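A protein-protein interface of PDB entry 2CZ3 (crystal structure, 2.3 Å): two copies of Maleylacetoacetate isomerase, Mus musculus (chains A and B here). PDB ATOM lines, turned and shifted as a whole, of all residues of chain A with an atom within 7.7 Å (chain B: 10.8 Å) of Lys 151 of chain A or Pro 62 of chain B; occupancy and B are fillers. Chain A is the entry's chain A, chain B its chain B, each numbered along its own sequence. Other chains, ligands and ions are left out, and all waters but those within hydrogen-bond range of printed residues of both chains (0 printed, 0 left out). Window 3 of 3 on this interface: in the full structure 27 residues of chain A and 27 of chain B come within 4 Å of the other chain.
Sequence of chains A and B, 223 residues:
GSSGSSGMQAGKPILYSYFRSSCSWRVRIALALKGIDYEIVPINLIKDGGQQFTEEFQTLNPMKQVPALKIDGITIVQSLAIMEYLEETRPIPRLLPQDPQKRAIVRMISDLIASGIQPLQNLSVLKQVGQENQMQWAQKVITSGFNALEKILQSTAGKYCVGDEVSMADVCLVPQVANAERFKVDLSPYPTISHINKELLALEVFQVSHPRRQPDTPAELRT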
ATOM      1  N   MET A 108      20.279  35.178 -10.518  1.00  0.00           N
ATOM      2  CA  MET A 108      20.702  33.955 -11.227  1.00  0.00           C
ATOM      3  C   MET A 108      21.634  34.266 -12.365  1.00  0.00           C
ATOM      4  O   MET A 108      22.717  33.688 -12.455  1.00  0.00           O
ATOM      5  CB  MET A 108      19.513  33.264 -11.846  1.00  0.00           C
ATOM      6  CG  MET A 108      18.850  32.305 -10.967  1.00  0.00           C
ATOM      7  SD  MET A 108      17.142  31.872 -11.740  1.00  0.00           S
ATOM      8  CE  MET A 108      17.649  30.927 -13.309  1.00  0.00           C
ATOM      9  N   LEU A 112      25.537  33.555 -12.661  1.00  0.00           N
ATOM     10  CA  LEU A 112      25.940  32.701 -13.783  1.00  0.00           C
ATOM     11  C   LEU A 112      27.138  33.307 -14.509  1.00  0.00           C
ATOM     12  O   LEU A 112      28.079  32.623 -14.870  1.00  0.00           O
ATOM     13  CB  LEU A 112      24.772  32.583 -14.754  1.00  0.00           C
ATOM     14  CG  LEU A 112      24.631  31.303 -15.556  1.00  0.00           C
ATOM     15  CD1 LEU A 112      23.194  31.207 -16.113  1.00  0.00           C
ATOM     16  CD2 LEU A 112      25.654  31.265 -16.660  1.00  0.00           C
ATOM     17  N   SER A 144      29.731  27.791 -23.872  1.00  0.00           N
ATOM     18  CA  SER A 144      28.933  26.958 -22.959  1.00  0.00           C
ATOM     19  C   SER A 144      28.003  27.772 -22.085  1.00  0.00           C
ATOM     20  O   SER A 144      26.828  27.424 -21.963  1.00  0.00           O
ATOM     21  CB  SER A 144      29.841  26.122 -22.040  1.00  0.00           C
ATOM     22  OG  SER A 144      30.393  25.017 -22.734  1.00  0.00           O
ATOM     23  N   GLY A 145      28.533  28.821 -21.445  1.00  0.00           N
ATOM     24  CA  GLY A 145      27.709  29.733 -20.671  1.00  0.00           C
ATOM     25  C   GLY A 145      26.666  30.472 -21.525  1.00  0.00           C
ATOM     26  O   GLY A 145      25.518  30.624 -21.123  1.00  0.00           O
ATOM     27  N   PHE A 146      27.070  30.932 -22.707  1.00  0.00           N
ATOM     28  CA  PHE A 146      26.193  31.707 -23.597  1.00  0.00           C
ATOM     29  C   PHE A 146      25.101  30.838 -24.206  1.00  0.00           C
ATOM     30  O   PHE A 146      24.031  31.326 -24.553  1.00  0.00           O
ATOM     31  CB  PHE A 146      27.027  32.391 -24.700  1.00  0.00           C
ATOM     32  CG  PHE A 146      27.699  33.699 -24.265  1.00  0.00           C
ATOM     33  CD1 PHE A 146      27.836  34.045 -22.921  1.00  0.00           C
ATOM     34  CD2 PHE A 146      28.172  34.580 -25.209  1.00  0.00           C
ATOM     35  CE1 PHE A 146      28.442  35.255 -22.543  1.00  0.00           C
ATOM     36  CE2 PHE A 146      28.771  35.789 -24.836  1.00  0.00           C
ATOM     37  CZ  PHE A 146      28.907  36.127 -23.514  1.00  0.00           C
ATOM     38  N   ASN A 147      25.383  29.545 -24.320  1.00  0.00           N
ATOM     39  CA  ASN A 147      24.402  28.553 -24.733  1.00  0.00           C
ATOM     40  C   ASN A 147      23.335  28.455 -23.663  1.00  0.00           C
ATOM     41  O   ASN A 147      22.162  28.350 -23.970  1.00  0.00           O
ATOM     42  CB  ASN A 147      25.078  27.182 -24.945  1.00  0.00           C
ATOM     43  CG  ASN A 147      26.031  27.168 -26.132  1.00  0.00           C
ATOM     44  OD1 ASN A 147      26.978  26.368 -26.187  1.00  0.00           O
ATOM     45  ND2 ASN A 147      25.794  28.047 -27.087  1.00  0.00           N
ATOM     46  N   ALA A 148      23.750  28.493 -22.405  1.00  0.00           N
ATOM     47  CA  ALA A 148      22.818  28.460 -21.298  1.00  0.00           C
ATOM     48  C   ALA A 148      22.034  29.772 -21.167  1.00  0.00           C
ATOM     49  O   ALA A 148      20.815  29.782 -21.077  1.00  0.00           O
ATOM     50  CB  ALA A 148      23.578  28.148 -20.049  1.00  0.00           C
ATOM     51  N   LEU A 149      22.757  30.877 -21.201  1.00  0.00           N
ATOM     52  CA  LEU A 149      22.219  32.204 -20.906  1.00  0.00           C
ATOM     53  C   LEU A 149      21.234  32.680 -21.968  1.00  0.00           C
ATOM     54  O   LEU A 149      20.184  33.269 -21.664  1.00  0.00           O
ATOM     55  CB  LEU A 149      23.406  33.166 -20.799  1.00  0.00           C
ATOM     56  CG  LEU A 149      23.202  34.619 -20.442  1.00  0.00           C
ATOM     57  CD1 LEU A 149      22.204  34.791 -19.302  1.00  0.00           C
ATOM     58  CD2 LEU A 149      24.571  35.231 -20.108  1.00  0.00           C
ATOM     59  N   GLU A 150      21.573  32.403 -23.224  1.00  0.00           N
ATOM     60  CA  GLU A 150      20.702  32.701 -24.363  1.00  0.00           C
ATOM     61  C   GLU A 150      19.363  31.994 -24.216  1.00  0.00           C
ATOM     62  O   GLU A 150      18.338  32.553 -24.590  1.00  0.00           O
ATOM     63  CB  GLU A 150      21.414  32.282 -25.658  1.00  0.00           C
ATOM     64  CG  GLU A 150      20.646  32.349 -26.970  1.00  0.00           C
ATOM     65  CD  GLU A 150      20.414  33.768 -27.450  1.00  0.00           C
ATOM     66  OE1 GLU A 150      21.208  34.673 -27.089  1.00  0.00           O
ATOM     67  OE2 GLU A 150      19.425  33.974 -28.187  1.00  0.00           O
ATOM     68  N   LYS A 151      19.365  30.766 -23.690  1.00  0.00           N
ATOM     69  CA  LYS A 151      18.112  30.014 -23.516  1.00  0.00           C
ATOM     70  C   LYS A 151      17.262  30.573 -22.374  1.00  0.00           C
ATOM     71  O   LYS A 151      16.041  30.652 -22.463  1.00  0.00           O
ATOM     72  CB  LYS A 151      18.379  28.521 -23.308  1.00  0.00           C
ATOM     73  CG  LYS A 151      18.815  27.778 -24.590  1.00  0.00           C
ATOM     74  CD  LYS A 151      19.464  26.405 -24.257  1.00  0.00           C
ATOM     75  CE  LYS A 151      19.915  25.661 -25.495  1.00  0.00           C
ATOM     76  NZ  LYS A 151      20.896  24.589 -25.149  1.00  0.00           N
ATOM     77  N   ILE A 152      17.925  30.972 -21.304  1.00  0.00           N
ATOM     78  CA  ILE A 152      17.274  31.599 -20.165  1.00  0.00           C
ATOM     79  C   ILE A 152      16.619  32.901 -20.587  1.00  0.00           C
ATOM     80  O   ILE A 152      15.480  33.182 -20.188  1.00  0.00           O
ATOM     81  CB  ILE A 152      18.319  31.818 -19.067  1.00  0.00           C
ATOM     82  CG1 ILE A 152      18.798  30.449 -18.559  1.00  0.00           C
ATOM     83  CG2 ILE A 152      17.758  32.674 -17.923  1.00  0.00           C
ATOM     84  CD1 ILE A 152      20.074  30.470 -17.742  1.00  0.00           C
ATOM     85  N   LEU A 153      17.322  33.673 -21.418  1.00  0.00           N
ATOM     86  CA  LEU A 153      16.847  34.979 -21.874  1.00  0.00           C
ATOM     87  C   LEU A 153      15.647  34.865 -22.812  1.00  0.00           C
ATOM     88  O   LEU A 153      14.866  35.806 -22.925  1.00  0.00           O
ATOM     89  CB  LEU A 153      17.982  35.772 -22.534  1.00  0.00           C
ATOM     90  CG  LEU A 153      19.209  36.035 -21.645  1.00  0.00           C
ATOM     91  CD1 LEU A 153      20.309  36.702 -22.407  1.00  0.00           C
ATOM     92  CD2 LEU A 153      18.881  36.858 -20.422  1.00  0.00           C
ATOM     93  N   GLN A 154      15.472  33.716 -23.461  1.00  0.00           N
ATOM     94  CA  GLN A 154      14.247  33.489 -24.244  1.00  0.00           C
ATOM     95  C   GLN A 154      13.009  33.623 -23.363  1.00  0.00           C
ATOM     96  O   GLN A 154      11.933  33.972 -23.857  1.00  0.00           O
ATOM     97  CB  GLN A 154      14.182  32.087 -24.891  1.00  0.00           C
ATOM     98  CG  GLN A 154      15.161  31.766 -26.036  1.00  0.00           C
ATOM     99  CD  GLN A 154      15.362  32.907 -27.006  1.00  0.00           C
ATOM    100  OE1 GLN A 154      14.565  33.098 -27.944  1.00  0.00           O
ATOM    101  NE2 GLN A 154      16.428  33.665 -26.798  1.00  0.00           N
ATOM    102  N   SER A 155      13.149  33.306 -22.076  1.00  0.00           N
ATOM    103  CA  SER A 155      12.031  33.399 -21.127  1.00  0.00           C
ATOM    104  C   SER A 155      11.955  34.736 -20.407  1.00  0.00           C
ATOM    105  O   SER A 155      10.859  35.219 -20.143  1.00  0.00           O
ATOM    106  CB  SER A 155      12.105  32.300 -20.068  1.00  0.00           C
ATOM    107  OG  SER A 155      12.168  31.022 -20.661  1.00  0.00           O
ATOM    108  N   THR A 156      13.104  35.331 -20.099  1.00  0.00           N
ATOM    109  CA  THR A 156      13.158  36.454 -19.159  1.00  0.00           C
ATOM    110  C   THR A 156      13.214  37.825 -19.811  1.00  0.00           C
ATOM    111  O   THR A 156      12.722  38.808 -19.243  1.00  0.00           O
ATOM    112  CB  THR A 156      14.381  36.303 -18.248  1.00  0.00           C
ATOM    113  OG1 THR A 156      15.570  36.278 -19.035  1.00  0.00           O
ATOM    114  CG2 THR A 156      14.379  34.944 -17.533  1.00  0.00           C
ATOM    115  N   TYR A 190      23.786  33.822 -30.769  1.00  0.00           N
ATOM    116  CA  TYR A 190      23.248  34.396 -29.544  1.00  0.00           C
ATOM    117  C   TYR A 190      22.572  35.736 -29.833  1.00  0.00           C
ATOM    118  O   TYR A 190      23.057  36.796 -29.395  1.00  0.00           O
ATOM    119  CB  TYR A 190      24.404  34.562 -28.546  1.00  0.00           C
ATOM    120  CG  TYR A 190      25.295  33.330 -28.410  1.00  0.00           C
ATOM    121  CD1 TYR A 190      26.648  33.364 -28.758  1.00  0.00           C
ATOM    122  CD2 TYR A 190      24.784  32.138 -27.906  1.00  0.00           C
ATOM    123  CE1 TYR A 190      27.468  32.242 -28.604  1.00  0.00           C
ATOM    124  CE2 TYR A 190      25.599  31.001 -27.747  1.00  0.00           C
ATOM    125  CZ  TYR A 190      26.933  31.063 -28.098  1.00  0.00           C
ATOM    126  OH  TYR A 190      27.710  29.947 -27.945  1.00  0.00           O
ATOM    127  N   THR A 192      19.610  37.113 -28.926  1.00  0.00           N
ATOM    128  CA  THR A 192      19.064  37.813 -27.752  1.00  0.00           C
ATOM    129  C   THR A 192      20.138  38.501 -26.939  1.00  0.00           C
ATOM    130  O   THR A 192      19.953  39.623 -26.504  1.00  0.00           O
ATOM    131  CB  THR A 192      18.325  36.839 -26.838  1.00  0.00           C
ATOM    132  OG1 THR A 192      17.445  36.018 -27.617  1.00  0.00           O
ATOM    133  CG2 THR A 192      17.431  37.582 -25.831  1.00  0.00           C
ATOM    134  N   ILE A 193      21.244  37.807 -26.702  1.00  0.00           N
ATOM    135  CA  ILE A 193      22.371  38.372 -25.945  1.00  0.00           C
ATOM    136  C   ILE A 193      22.917  39.562 -26.702  1.00  0.00           C
ATOM    137  O   ILE A 193      23.189  40.582 -26.113  1.00  0.00           O
ATOM    138  CB  ILE A 193      23.477  37.308 -25.697  1.00  0.00           C
ATOM    139  CG1 ILE A 193      23.042  36.345 -24.599  1.00  0.00           C
ATOM    140  CG2 ILE A 193      24.829  37.948 -25.340  1.00  0.00           C
ATOM    141  CD1 ILE A 193      23.903  35.076 -24.468  1.00  0.00           C
ATOM    142  N   THR B  54      13.376  15.447 -16.242  1.00  0.00           N
ATOM    143  CA  THR B  54      14.432  16.143 -16.979  1.00  0.00           C
ATOM    144  C   THR B  54      13.976  17.533 -17.441  1.00  0.00           C
ATOM    145  O   THR B  54      14.745  18.491 -17.353  1.00  0.00           O
ATOM    146  CB  THR B  54      14.890  15.296 -18.197  1.00  0.00           C
ATOM    147  OG1 THR B  54      15.131  13.935 -17.794  1.00  0.00           O
ATOM    148  CG2 THR B  54      16.244  15.781 -18.735  1.00  0.00           C
ATOM    149  N   GLU B  55      12.730  17.623 -17.928  1.00  0.00           N
ATOM    150  CA  GLU B  55      12.096  18.891 -18.332  1.00  0.00           C
ATOM    151  C   GLU B  55      12.152  19.884 -17.178  1.00  0.00           C
ATOM    152  O   GLU B  55      12.698  20.975 -17.345  1.00  0.00           O
ATOM    153  CB  GLU B  55      10.621  18.688 -18.778  1.00  0.00           C
ATOM    154  CG  GLU B  55      10.297  19.072 -20.233  1.00  0.00           C
ATOM    155  CD  GLU B  55       9.352  18.087 -20.945  1.00  0.00           C
ATOM    156  OE1 GLU B  55       8.179  18.459 -21.226  1.00  0.00           O
ATOM    157  OE2 GLU B  55       9.779  16.939 -21.236  1.00  0.00           O
ATOM    158  N   GLU B  56      11.610  19.480 -16.020  1.00  0.00           N
ATOM    159  CA  GLU B  56      11.550  20.315 -14.803  1.00  0.00           C
ATOM    160  C   GLU B  56      12.947  20.745 -14.334  1.00  0.00           C
ATOM    161  O   GLU B  56      13.191  21.921 -14.022  1.00  0.00           O
ATOM    162  CB  GLU B  56      10.844  19.569 -13.649  1.00  0.00           C
ATOM    163  CG  GLU B  56       9.360  19.286 -13.865  1.00  0.00           C
ATOM    164  CD  GLU B  56       8.822  18.166 -12.978  1.00  0.00           C
ATOM    165  OE1 GLU B  56       9.615  17.299 -12.539  1.00  0.00           O
ATOM    166  OE2 GLU B  56       7.597  18.152 -12.719  1.00  0.00           O
ATOM    167  N   PHE B  57      13.860  19.780 -14.285  1.00  0.00           N
ATOM    168  CA  PHE B  57      15.224  20.046 -13.859  1.00  0.00           C
ATOM    169  C   PHE B  57      15.817  21.162 -14.704  1.00  0.00           C
ATOM    170  O   PHE B  57      16.354  22.138 -14.180  1.00  0.00           O
ATOM    171  CB  PHE B  57      16.084  18.781 -13.970  1.00  0.00           C
ATOM    172  CG  PHE B  57      17.503  18.965 -13.491  1.00  0.00           C
ATOM    173  CD1 PHE B  57      17.776  19.661 -12.311  1.00  0.00           C
ATOM    174  CD2 PHE B  57      18.564  18.449 -14.223  1.00  0.00           C
ATOM    175  CE1 PHE B  57      19.081  19.838 -11.874  1.00  0.00           C
ATOM    176  CE2 PHE B  57      19.872  18.619 -13.795  1.00  0.00           C
ATOM    177  CZ  PHE B  57      20.133  19.312 -12.615  1.00  0.00           C
ATOM    178  N   GLN B  58      15.649  21.017 -16.017  1.00  0.00           N
ATOM    179  CA  GLN B  58      16.243  21.900 -17.013  1.00  0.00           C
ATOM    180  C   GLN B  58      15.424  23.148 -17.364  1.00  0.00           C
ATOM    181  O   GLN B  58      15.848  23.907 -18.231  1.00  0.00           O
ATOM    182  CB  GLN B  58      16.513  21.107 -18.299  1.00  0.00           C
ATOM    183  CG  GLN B  58      17.426  19.901 -18.104  1.00  0.00           C
ATOM    184  CD  GLN B  58      18.688  19.975 -18.922  1.00  0.00           C
ATOM    185  OE1 GLN B  58      19.373  21.007 -18.931  1.00  0.00           O
ATOM    186  NE2 GLN B  58      19.015  18.880 -19.605  1.00  0.00           N
ATOM    187  N   THR B  59      14.273  23.382 -16.723  1.00  0.00           N
ATOM    188  CA  THR B  59      13.566  24.651 -16.962  1.00  0.00           C
ATOM    189  C   THR B  59      14.345  25.718 -16.219  1.00  0.00           C
ATOM    190  O   THR B  59      14.668  25.562 -15.037  1.00  0.00           O
ATOM    191  CB  THR B  59      12.053  24.694 -16.538  1.00  0.00           C
ATOM    192  OG1 THR B  59      11.935  24.967 -15.141  1.00  0.00           O
ATOM    193  CG2 THR B  59      11.339  23.392 -16.741  1.00  0.00           C
ATOM    194  N   LEU B  60      14.668  26.784 -16.949  1.00  0.00           N
ATOM    195  CA  LEU B  60      15.525  27.862 -16.455  1.00  0.00           C
ATOM    196  C   LEU B  60      16.860  27.319 -15.941  1.00  0.00           C
ATOM    197  O   LEU B  60      17.505  27.929 -15.105  1.00  0.00           O
ATOM    198  CB  LEU B  60      14.783  28.712 -15.409  1.00  0.00           C
ATOM    199  CG  LEU B  60      13.924  29.815 -16.046  1.00  0.00           C
ATOM    200  CD1 LEU B  60      14.802  30.815 -16.788  1.00  0.00           C
ATOM    201  CD2 LEU B  60      12.842  29.254 -17.006  1.00  0.00           C
ATOM    202  N   ASN B  61      17.269  26.176 -16.490  1.00  0.00           N
ATOM    203  CA  ASN B  61      18.529  25.540 -16.150  1.00  0.00           C
ATOM    204  C   ASN B  61      19.015  24.644 -17.291  1.00  0.00           C
ATOM    205  O   ASN B  61      19.216  23.429 -17.110  1.00  0.00           O
ATOM    206  CB  ASN B  61      18.398  24.726 -14.862  1.00  0.00           C
ATOM    207  CG  ASN B  61      19.733  24.181 -14.378  1.00  0.00           C
ATOM    208  OD1 ASN B  61      20.800  24.743 -14.677  1.00  0.00           O
ATOM    209  ND2 ASN B  61      19.683  23.090 -13.618  1.00  0.00           N
ATOM    210  N   PRO B  62      19.240  25.241 -18.459  1.00  0.00           N
ATOM    211  CA  PRO B  62      19.728  24.485 -19.617  1.00  0.00           C
ATOM    212  C   PRO B  62      21.127  23.867 -19.407  1.00  0.00           C
ATOM    213  O   PRO B  62      21.552  23.037 -20.209  1.00  0.00           O
ATOM    214  CB  PRO B  62      19.774  25.541 -20.725  1.00  0.00           C
ATOM    215  CG  PRO B  62      18.950  26.682 -20.220  1.00  0.00           C
ATOM    216  CD  PRO B  62      19.073  26.672 -18.765  1.00  0.00           C
ATOM    217  N   MET B  63      21.816  24.271 -18.337  1.00  0.00           N
ATOM    218  CA  MET B  63      23.167  23.781 -18.026  1.00  0.00           C
ATOM    219  C   MET B  63      23.211  22.535 -17.103  1.00  0.00           C
ATOM    220  O   MET B  63      24.294  22.133 -16.679  1.00  0.00           O
ATOM    221  CB  MET B  63      24.018  24.924 -17.437  1.00  0.00           C
ATOM    222  CG  MET B  63      23.364  25.682 -16.282  1.00  0.00           C
ATOM    223  SD  MET B  63      22.336  27.107 -16.783  1.00  0.00           S
ATOM    224  CE  MET B  63      23.590  28.179 -16.986  1.00  0.00           C
ATOM    225  N   LYS B  64      22.054  21.923 -16.816  1.00  0.00           N
ATOM    226  CA  LYS B  64      21.958  20.712 -15.972  1.00  0.00           C
ATOM    227  C   LYS B  64      22.671  20.914 -14.623  1.00  0.00           C
ATOM    228  O   LYS B  64      23.363  20.045 -14.105  1.00  0.00           O
ATOM    229  CB  LYS B  64      22.501  19.474 -16.711  1.00  0.00           C
ATOM    230  CG  LYS B  64      21.522  18.827 -17.715  1.00  0.00           C
ATOM    231  CD  LYS B  64      22.007  17.427 -18.168  1.00  0.00           C
ATOM    232  CE  LYS B  64      21.508  17.061 -19.581  1.00  0.00           C
ATOM    233  NZ  LYS B  64      22.355  16.064 -20.315  1.00  0.00           N
ATOM    234  N   GLN B  65      22.431  22.080 -14.055  1.00  0.00           N
ATOM    235  CA  GLN B  65      23.159  22.602 -12.916  1.00  0.00           C
ATOM    236  C   GLN B  65      22.486  22.259 -11.600  1.00  0.00           C
ATOM    237  O   GLN B  65      21.261  22.192 -11.505  1.00  0.00           O
ATOM    238  CB  GLN B  65      23.295  24.136 -13.006  1.00  0.00           C
ATOM    239  CG  GLN B  65      24.565  24.679 -12.388  1.00  0.00           C
ATOM    240  CD  GLN B  65      24.723  26.180 -12.562  1.00  0.00           C
ATOM    241  OE1 GLN B  65      24.356  26.952 -11.667  1.00  0.00           O
ATOM    242  NE2 GLN B  65      25.300  26.597 -13.688  1.00  0.00           N
ATOM    243  N   VAL B  66      23.325  22.075 -10.592  1.00  0.00           N
ATOM    244  CA  VAL B  66      22.894  21.946  -9.203  1.00  0.00           C
ATOM    245  C   VAL B  66      23.703  22.929  -8.336  1.00  0.00           C
ATOM    246  O   VAL B  66      24.876  23.196  -8.641  1.00  0.00           O
ATOM    247  CB  VAL B  66      23.071  20.487  -8.666  1.00  0.00           C
ATOM    248  CG1 VAL B  66      22.197  19.477  -9.469  1.00  0.00           C
ATOM    249  CG2 VAL B  66      24.551  20.064  -8.662  1.00  0.00           C
ATOM    250  N   PRO B  67      23.084  23.484  -7.285  1.00  0.00           N
ATOM    251  CA  PRO B  67      21.676  23.236  -6.956  1.00  0.00           C
ATOM    252  C   PRO B  67      20.654  23.965  -7.835  1.00  0.00           C
ATOM    253  O   PRO B  67      20.923  25.005  -8.441  1.00  0.00           O
ATOM    254  CB  PRO B  67      21.546  23.723  -5.498  1.00  0.00           C
ATOM    255  CG  PRO B  67      22.667  24.700  -5.286  1.00  0.00           C
ATOM    256  CD  PRO B  67      23.711  24.410  -6.327  1.00  0.00           C
ATOM    257  N   ALA B  68      19.470  23.371  -7.908  1.00  0.00           N
ATOM    258  CA  ALA B  68      18.282  24.050  -8.431  1.00  0.00           C
ATOM    259  C   ALA B  68      17.168  23.869  -7.419  1.00  0.00           C
ATOM    260  O   ALA B  68      17.048  22.822  -6.802  1.00  0.00           O
ATOM    261  CB  ALA B  68      17.870  23.506  -9.811  1.00  0.00           C
ATOM    262  N   THR B  75      11.592  28.606 -10.294  1.00  0.00           N
ATOM    263  CA  THR B  75      12.848  27.881 -10.284  1.00  0.00           C
ATOM    264  C   THR B  75      14.021  28.836 -10.144  1.00  0.00           C
ATOM    265  O   THR B  75      14.137  29.815 -10.905  1.00  0.00           O
ATOM    266  CB  THR B  75      13.013  27.159 -11.605  1.00  0.00           C
ATOM    267  OG1 THR B  75      11.799  26.469 -11.930  1.00  0.00           O
ATOM    268  CG2 THR B  75      14.102  26.091 -11.485  1.00  0.00           C
ATOM    269  N   ILE B  76      14.922  28.520  -9.221  1.00  0.00           N
ATOM    270  CA  ILE B  76      16.080  29.345  -8.977  1.00  0.00           C
ATOM    271  C   ILE B  76      17.325  28.484  -8.964  1.00  0.00           C
ATOM    272  O   ILE B  76      17.433  27.550  -8.167  1.00  0.00           O
ATOM    273  CB  ILE B  76      15.968  30.126  -7.642  1.00  0.00           C
ATOM    274  CG1 ILE B  76      14.566  30.695  -7.437  1.00  0.00           C
ATOM    275  CG2 ILE B  76      16.975  31.275  -7.623  1.00  0.00           C
ATOM    276  CD1 ILE B  76      14.388  31.371  -6.082  1.00  0.00           C
ATOM    277  N   VAL B  77      18.263  28.808  -9.851  1.00  0.00           N
ATOM    278  CA  VAL B  77      19.604  28.216  -9.831  1.00  0.00           C
ATOM    279  C   VAL B  77      20.584  29.239  -9.278  1.00  0.00           C
ATOM    280  O   VAL B  77      20.258  30.423  -9.152  1.00  0.00           O
ATOM    281  CB  VAL B  77      20.079  27.750 -11.232  1.00  0.00           C
ATOM    282  CG1 VAL B  77      19.123  26.710 -11.778  1.00  0.00           C
ATOM    283  CG2 VAL B  77      20.232  28.932 -12.209  1.00  0.00           C
ATOM    284  N   GLN B  78      21.787  28.774  -8.964  1.00  0.00           N
ATOM    285  CA  GLN B  78      22.825  29.604  -8.377  1.00  0.00           C
ATOM    286  C   GLN B  78      22.566  29.777  -6.887  1.00  0.00           C
ATOM    287  O   GLN B  78      21.685  30.536  -6.487  1.00  0.00           O
ATOM    288  CB  GLN B  78      22.903  30.993  -9.057  1.00  0.00           C
ATOM    289  CG  GLN B  78      23.479  30.969 -10.450  1.00  0.00           C
ATOM    290  CD  GLN B  78      24.926  30.508 -10.448  1.00  0.00           C
ATOM    291  OE1 GLN B  78      25.723  30.964  -9.620  1.00  0.00           O
ATOM    292  NE2 GLN B  78      25.266  29.595 -11.358  1.00  0.00           N
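O of Thr 75 of chain B sits close to SD of Met 108 of chain A (3.7 Å).
The backbone NH (N) of Val 77 of chain B sits close to the side-chain sulfur (SD) of Met 108 of chain A (3.8 Å).
The side-chain amide oxygen (OE1) of Gln 58 of chain B sits close to the backbone carbonyl oxygen (O) of Pro 62 of chain B (3.2 Å).
The side-chain sulfur (SD) of Met 63 of chain B sits close to the side-chain amide oxygen (OD1) of Asn 61 of chain B (3.5 Å).
The side-chain amide nitrogen (NE2) of Gln 78 of chain B is in hydrogen-bond range of the side-chain amide oxygen (OE1) of Gln 65 of chain B (2.8 Å).
The backbone carbonyl oxygen (O) of Ile 152 of chain A sits at hydrogen-bond distance from the side-chain hydroxyl (OG1) of Thr 156 of chain A (3.3 Å).
Among the printed residues, merely in contact across the chains: Met 108 of chain A with Leu 60 of chain B (3.5 Å), Met 108 of chain A with Ile 76 of chain B (3.9 Å), Met 108 of chain A with Gln 78 of chain B (3.5 Å), Leu 112 of chain A with Met 63 of chain B (3.2 Å), Leu 112 of chain A with Gln 78 of chain B (3.8 Å), Ala 148 of chain A with Pro 62 of chain B (3.7 Å), Ala 148 of chain A with Met 63 of chain B (3.1 Å), Lys 151 of chain A with Pro 62 of chain B (3.6 Å), Ile 152 of chain A with Leu 60 of chain B (3.7 Å) and Ile 152 of chain A with Pro 62 of chain B (3.8 Å).
Printed residues of chain B within 4 Å of Met 108 of chain A: Leu 60, Thr 75, Ile 76, Val 77 and Gln 78.
No residue of chain B comes within 4 Å of Asn 147 of chain A.
Ala 148 of chain A touches just these residues of chain B: Pro 62 and Met 63.
No residue of chain B comes within 4 Å of Glu 150 of chain A.
Lys 151 of chain A touches one residue of chain B.
Of the printed residues of chain B, Ile 152 of chain A touches Leu 60 (3.7 Å) and Pro 62 (3.8 Å).
No residue of chain B comes within 4 Å of Gln 154 of chain A.
Of the printed residues of chain A, Pro 62 of chain B touches Ala 148, Lys 151 and Ile 152.
Printed residues of chain A within 4 Å of Met 63 of chain B: Leu 112 and Ala 148.
The nearest residue of chain B that does not touch Lys 151 of chain A is Leu 60 of chain B (5.8 Å).
The nearest printed residue of chain A that does not touch Leu 60 of chain B is Ser 155 of chain A (4.1 Å).
Hydrophobic or aromatic side chains of chain A that line the printed part of chain B: Met 108, Leu 112, Ala 148 and Ile 152.
Along chain A the printed residues that touch a printed residue of chain B span positions 108 to 152.
Printed residues of chain B that touch a printed residue of chain A: Leu 60, Pro 62, Met 63, Thr 75, Ile 76, Val 77 and Gln 78.
Among the printed residues, no Asp or Glu carboxylate lies within 4 Å of a Lys or Arg side-chain nitrogen of the other chain.
No position is printed for both chains.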
